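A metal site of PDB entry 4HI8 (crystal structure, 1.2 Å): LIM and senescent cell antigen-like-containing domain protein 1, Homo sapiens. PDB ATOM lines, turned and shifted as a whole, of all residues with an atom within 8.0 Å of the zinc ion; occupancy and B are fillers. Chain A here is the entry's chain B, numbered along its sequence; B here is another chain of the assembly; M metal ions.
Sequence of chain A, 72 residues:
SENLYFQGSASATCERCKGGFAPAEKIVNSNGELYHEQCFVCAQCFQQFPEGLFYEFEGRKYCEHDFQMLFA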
ATOM      1  N   THR A  13      17.503   1.749  13.106  1.00  0.00           N
ATOM      2  CA  THR A  13      18.228   0.653  13.746  1.00  0.00           C
ATOM      3  C   THR A  13      17.302  -0.501  14.044  1.00  0.00           C
ATOM      4  O   THR A  13      16.094  -0.351  14.208  1.00  0.00           O
ATOM      5  CB  THR A  13      18.899   1.093  15.087  1.00  0.00           C
ATOM      6  OG1 THR A  13      17.892   1.655  15.953  1.00  0.00           O
ATOM      7  CG2 THR A  13      20.026   2.115  14.840  1.00  0.00           C
ATOM      8  N   CYS A  14      17.916  -1.674  14.114  1.00  0.00           N
ATOM      9  CA  CYS A  14      17.249  -2.900  14.532  1.00  0.00           C
ATOM     10  C   CYS A  14      16.871  -2.818  15.990  1.00  0.00           C
ATOM     11  O   CYS A  14      17.739  -2.591  16.827  1.00  0.00           O
ATOM     12  CB  CYS A  14      18.182  -4.100  14.298  1.00  0.00           C
ATOM     13  SG  CYS A  14      17.545  -5.645  14.899  1.00  0.00           S
ATOM     14  N   GLU A  15      15.598  -3.111  16.315  1.00  0.00           N
ATOM     15  CA  GLU A  15      15.077  -3.065  17.680  1.00  0.00           C
ATOM     16  C   GLU A  15      15.842  -4.041  18.625  1.00  0.00           C
ATOM     17  O   GLU A  15      16.033  -3.764  19.819  1.00  0.00           O
ATOM     18  CB  GLU A  15      13.557  -3.344  17.680  1.00  0.00           C
ATOM     19  CG  GLU A  15      12.920  -3.584  19.028  1.00  0.00           C
ATOM     20  CD  GLU A  15      12.847  -2.357  19.913  1.00  0.00           C
ATOM     21  OE1 GLU A  15      12.522  -1.246  19.416  1.00  0.00           O
ATOM     22  OE2 GLU A  15      13.123  -2.475  21.121  1.00  0.00           O
ATOM     23  N   ARG A  16      16.300  -5.168  18.108  1.00  0.00           N
ATOM     24  CA  ARG A  16      16.987  -6.146  18.954  1.00  0.00           C
ATOM     25  C   ARG A  16      18.453  -5.795  19.156  1.00  0.00           C
ATOM     26  O   ARG A  16      18.891  -5.758  20.307  1.00  0.00           O
ATOM     27  CB  ARG A  16      16.901  -7.542  18.385  1.00  0.00           C
ATOM     28  CG  ARG A  16      17.362  -8.592  19.412  1.00  0.00           C
ATOM     29  CD  ARG A  16      17.657  -9.986  18.800  1.00  0.00           C
ATOM     30  NE  ARG A  16      18.931  -9.982  18.077  1.00  0.00           N
ATOM     31  CZ  ARG A  16      20.124 -10.144  18.671  1.00  0.00           C
ATOM     32  NH1 ARG A  16      20.213 -10.208  20.014  1.00  0.00           N
ATOM     33  NH2 ARG A  16      21.227 -10.137  17.940  1.00  0.00           N
ATOM     34  N   CYS A  17      19.225  -5.595  18.066  1.00  0.00           N
ATOM     35  CA  CYS A  17      20.698  -5.518  18.172  1.00  0.00           C
ATOM     36  C   CYS A  17      21.236  -4.115  18.032  1.00  0.00           C
ATOM     37  O   CYS A  17      22.420  -3.888  18.258  1.00  0.00           O
ATOM     38  CB  CYS A  17      21.383  -6.412  17.120  1.00  0.00           C
ATOM     39  SG  CYS A  17      21.402  -5.775  15.410  1.00  0.00           S
ATOM     40  N   LYS A  18      20.369  -3.201  17.648  1.00  0.00           N
ATOM     41  CA  LYS A  18      20.701  -1.777  17.486  1.00  0.00           C
ATOM     42  C   LYS A  18      21.608  -1.472  16.306  1.00  0.00           C
ATOM     43  O   LYS A  18      22.095  -0.344  16.171  1.00  0.00           O
ATOM     44  CB  LYS A  18      21.270  -1.181  18.772  1.00  0.00           C
ATOM     45  CG  LYS A  18      20.531  -1.593  20.006  1.00  0.00           C
ATOM     46  CD  LYS A  18      19.050  -1.276  19.871  1.00  0.00           C
ATOM     47  CE  LYS A  18      18.297  -1.627  21.171  1.00  0.00           C
ATOM     48  NZ  LYS A  18      16.840  -1.291  21.069  1.00  0.00           N
ATOM     49  N   GLY A  19      21.838  -2.434  15.422  1.00  0.00           N
ATOM     50  CA  GLY A  19      22.621  -2.169  14.224  1.00  0.00           C
ATOM     51  C   GLY A  19      21.753  -1.587  13.127  1.00  0.00           C
ATOM     52  O   GLY A  19      20.513  -1.704  13.144  1.00  0.00           O
ATOM     53  N   GLY A  20      22.388  -0.936  12.157  1.00  0.00           N
ATOM     54  CA  GLY A  20      21.649  -0.342  11.067  1.00  0.00           C
ATOM     55  C   GLY A  20      21.437  -1.296   9.908  1.00  0.00           C
ATOM     56  O   GLY A  20      21.878  -2.472   9.952  1.00  0.00           O
ATOM     57  N   PHE A  21      20.736  -0.757   8.898  1.00  0.00           N
ATOM     58  CA  PHE A  21      20.314  -1.519   7.732  1.00  0.00           C
ATOM     59  C   PHE A  21      21.040  -1.043   6.465  1.00  0.00           C
ATOM     60  O   PHE A  21      21.511   0.100   6.390  1.00  0.00           O
ATOM     61  CB  PHE A  21      18.795  -1.423   7.539  1.00  0.00           C
ATOM     62  CG  PHE A  21      17.996  -1.868   8.758  1.00  0.00           C
ATOM     63  CD1 PHE A  21      18.027  -3.196   9.186  1.00  0.00           C
ATOM     64  CD2 PHE A  21      17.264  -0.951   9.488  1.00  0.00           C
ATOM     65  CE1 PHE A  21      17.288  -3.588  10.286  1.00  0.00           C
ATOM     66  CE2 PHE A  21      16.532  -1.336  10.585  1.00  0.00           C
ATOM     67  CZ  PHE A  21      16.562  -2.667  11.003  1.00  0.00           C
ATOM     68  N   GLU A  25      18.071  -4.012   1.904  1.00  0.00           N
ATOM     69  CA  GLU A  25      18.170  -5.178   2.801  1.00  0.00           C
ATOM     70  C   GLU A  25      16.780  -5.712   3.176  1.00  0.00           C
ATOM     71  O   GLU A  25      15.870  -4.940   3.472  1.00  0.00           O
ATOM     72  CB  GLU A  25      18.923  -4.832   4.073  1.00  0.00           C
ATOM     73  CG  GLU A  25      19.116  -6.076   4.967  1.00  0.00           C
ATOM     74  CD  GLU A  25      19.942  -5.795   6.213  1.00  0.00           C
ATOM     75  OE1 GLU A  25      20.453  -4.662   6.329  1.00  0.00           O
ATOM     76  OE2 GLU A  25      20.087  -6.716   7.063  1.00  0.00           O
ATOM     77  N   LEU A  34      11.465  -2.524  13.640  1.00  0.00           N
ATOM     78  CA  LEU A  34      12.214  -3.124  12.554  1.00  0.00           C
ATOM     79  C   LEU A  34      13.332  -4.006  13.055  1.00  0.00           C
ATOM     80  O   LEU A  34      14.009  -3.662  14.015  1.00  0.00           O
ATOM     81  CB  LEU A  34      12.782  -2.049  11.613  1.00  0.00           C
ATOM     82  CG  LEU A  34      11.805  -0.979  11.151  1.00  0.00           C
ATOM     83  CD1 LEU A  34      12.518   0.005  10.240  1.00  0.00           C
ATOM     84  CD2 LEU A  34      10.576  -1.553  10.423  1.00  0.00           C
ATOM     85  N   TYR A  35      13.551  -5.115  12.350  1.00  0.00           N
ATOM     86  CA  TYR A  35      14.555  -6.104  12.706  1.00  0.00           C
ATOM     87  C   TYR A  35      15.353  -6.600  11.516  1.00  0.00           C
ATOM     88  O   TYR A  35      14.782  -6.830  10.443  1.00  0.00           O
ATOM     89  CB  TYR A  35      13.877  -7.376  13.311  1.00  0.00           C
ATOM     90  CG  TYR A  35      13.136  -7.133  14.615  1.00  0.00           C
ATOM     91  CD1 TYR A  35      11.835  -6.653  14.599  1.00  0.00           C
ATOM     92  CD2 TYR A  35      13.742  -7.360  15.865  1.00  0.00           C
ATOM     93  CE1 TYR A  35      11.150  -6.393  15.766  1.00  0.00           C
ATOM     94  CE2 TYR A  35      13.056  -7.120  17.018  1.00  0.00           C
ATOM     95  CZ  TYR A  35      11.765  -6.654  16.963  1.00  0.00           C
ATOM     96  OH  TYR A  35      11.130  -6.414  18.143  1.00  0.00           O
ATOM     97  N   HIS A  36      16.634  -6.893  11.724  1.00  0.00           N
ATOM     98  CA  HIS A  36      17.319  -7.740  10.740  1.00  0.00           C
ATOM     99  C   HIS A  36      16.649  -9.125  10.683  1.00  0.00           C
ATOM    100  O   HIS A  36      16.069  -9.599  11.693  1.00  0.00           O
ATOM    101  CB  HIS A  36      18.784  -7.967  11.111  1.00  0.00           C
ATOM    102  CG  HIS A  36      19.584  -6.726  11.219  1.00  0.00           C
ATOM    103  ND1 HIS A  36      20.011  -6.189  12.430  1.00  0.00           N
ATOM    104  CD2 HIS A  36      20.030  -5.891  10.243  1.00  0.00           C
ATOM    105  CE1 HIS A  36      20.696  -5.085  12.180  1.00  0.00           C
ATOM    106  NE2 HIS A  36      20.736  -4.887  10.866  1.00  0.00           N
ATOM    107  N   GLU A  37      16.786  -9.831   9.558  1.00  0.00           N
ATOM    108  CA  GLU A  37      16.222 -11.188   9.482  1.00  0.00           C
ATOM    109  C   GLU A  37      16.778 -12.120  10.556  1.00  0.00           C
ATOM    110  O   GLU A  37      16.069 -12.973  11.093  1.00  0.00           O
ATOM    111  CB  GLU A  37      16.454 -11.816   8.099  1.00  0.00           C
ATOM    112  CG  GLU A  37      15.477 -11.365   7.067  1.00  0.00           C
ATOM    113  CD  GLU A  37      15.578 -12.173   5.800  1.00  0.00           C
ATOM    114  OE1 GLU A  37      14.541 -12.789   5.442  1.00  0.00           O
ATOM    115  OE2 GLU A  37      16.673 -12.176   5.168  1.00  0.00           O
ATOM    116  N   GLN A  38      18.082 -11.997  10.862  1.00  0.00           N
ATOM    117  CA  GLN A  38      18.759 -12.818  11.856  1.00  0.00           C
ATOM    118  C   GLN A  38      18.450 -12.356  13.272  1.00  0.00           C
ATOM    119  O   GLN A  38      18.876 -12.956  14.252  1.00  0.00           O
ATOM    120  CB  GLN A  38      20.266 -12.782  11.633  1.00  0.00           C
ATOM    121  CG  GLN A  38      20.892 -11.422  11.809  1.00  0.00           C
ATOM    122  CD  GLN A  38      20.982 -10.609  10.499  1.00  0.00           C
ATOM    123  OE1 GLN A  38      20.175 -10.762   9.557  1.00  0.00           O
ATOM    124  NE2 GLN A  38      22.012  -9.749  10.422  1.00  0.00           N
ATOM    125  N   CYS A  39      17.651 -11.297  13.394  1.00  0.00           N
ATOM    126  CA  CYS A  39      17.268 -10.774  14.720  1.00  0.00           C
ATOM    127  C   CYS A  39      15.813 -10.947  15.093  1.00  0.00           C
ATOM    128  O   CYS A  39      15.474 -10.870  16.284  1.00  0.00           O
ATOM    129  CB  CYS A  39      17.619  -9.304  14.817  1.00  0.00           C
ATOM    130  SG  CYS A  39      19.386  -9.010  14.780  1.00  0.00           S
ATOM    131  N   PHE A  40      14.937 -11.149  14.110  1.00  0.00           N
ATOM    132  CA  PHE A  40      13.561 -11.490  14.418  1.00  0.00           C
ATOM    133  C   PHE A  40      13.470 -13.001  14.547  1.00  0.00           C
ATOM    134  O   PHE A  40      12.964 -13.709  13.678  1.00  0.00           O
ATOM    135  CB  PHE A  40      12.576 -10.908  13.373  1.00  0.00           C
ATOM    136  CG  PHE A  40      11.134 -11.052  13.809  1.00  0.00           C
ATOM    137  CD1 PHE A  40      10.655 -10.343  14.908  1.00  0.00           C
ATOM    138  CD2 PHE A  40      10.276 -11.921  13.131  1.00  0.00           C
ATOM    139  CE1 PHE A  40       9.309 -10.499  15.319  1.00  0.00           C
ATOM    140  CE2 PHE A  40       8.972 -12.059  13.510  1.00  0.00           C
ATOM    141  CZ  PHE A  40       8.485 -11.336  14.585  1.00  0.00           C
ATOM    142  N   PHE B 114      25.275 -13.439  20.886  1.00  0.00           N
ATOM    143  CA  PHE B 114      23.961 -13.003  20.377  1.00  0.00           C
ATOM    144  C   PHE B 114      23.542 -11.662  20.975  1.00  0.00           C
ATOM    145  O   PHE B 114      22.984 -10.818  20.272  1.00  0.00           O
ATOM    146  CB  PHE B 114      22.927 -14.088  20.691  1.00  0.00           C
ATOM    147  CG  PHE B 114      21.568 -13.837  20.080  1.00  0.00           C
ATOM    148  CD1 PHE B 114      21.334 -13.921  18.706  1.00  0.00           C
ATOM    149  CD2 PHE B 114      20.498 -13.605  20.895  1.00  0.00           C
ATOM    150  CE1 PHE B 114      20.021 -13.726  18.195  1.00  0.00           C
ATOM    151  CE2 PHE B 114      19.185 -13.373  20.361  1.00  0.00           C
ATOM    152  CZ  PHE B 114      18.989 -13.453  19.025  1.00  0.00           C
ATOM    153  N   LYS B 146      27.713  -9.736  16.029  1.00  0.00           N
ATOM    154  CA  LYS B 146      27.919  -8.707  15.006  1.00  0.00           C
ATOM    155  C   LYS B 146      29.378  -8.691  14.614  1.00  0.00           C
ATOM    156  O   LYS B 146      30.218  -9.214  15.342  1.00  0.00           O
ATOM    157  CB  LYS B 146      27.549  -7.295  15.533  1.00  0.00           C
ATOM    158  CG  LYS B 146      26.037  -7.134  15.720  1.00  0.00           C
ATOM    159  CD  LYS B 146      25.585  -5.700  15.832  1.00  0.00           C
ATOM    160  CE  LYS B 146      25.632  -5.215  17.263  1.00  0.00           C
ATOM    161  NZ  LYS B 146      25.003  -3.871  17.464  1.00  0.00           N
HETATM  162 ZN    ZN M   1      19.592  -6.777  14.390  1.00  0.00          ZN
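A ring nitrogen (NE2) of His 36 lies within hydrogen-bond range of the backbone carbonyl oxygen (O) of Gly 20 (2.8 Å).
SG of Cys 39 sits close to NE of Arg 16, 3.5 Å away.
SG of Cys 17 sits close to N of Gly 19 (3.4 Å).
The backbone carbonyl oxygen (O) of Cys 17 is in hydrogen-bond range of the side-chain amino group (NZ) of Lys 146 of chain B (2.7 Å).
SG of Cys 14 sits close to N of Arg 16 (3.5 Å).
N of Cys 14 lies within hydrogen-bond range of O of Gly 19, 2.8 Å away.
A ring nitrogen (ND1) of His 36 is bound to the zinc ion, at 2.1 Å.
The zinc ion is bound by the side-chain sulfur (SG) of Cys 39.
The zinc ion is bound by SG of Cys 17, 2.3 Å away.
The side-chain sulfur (SG) of Cys 14 binds the zinc ion (2.4 Å).
Within 4 Å of the zinc ion: Cys 14, Cys 17, His 36 and Cys 39.
The nearest printed residue that does not touch the zinc ion is Arg 16 (4.9 Å).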
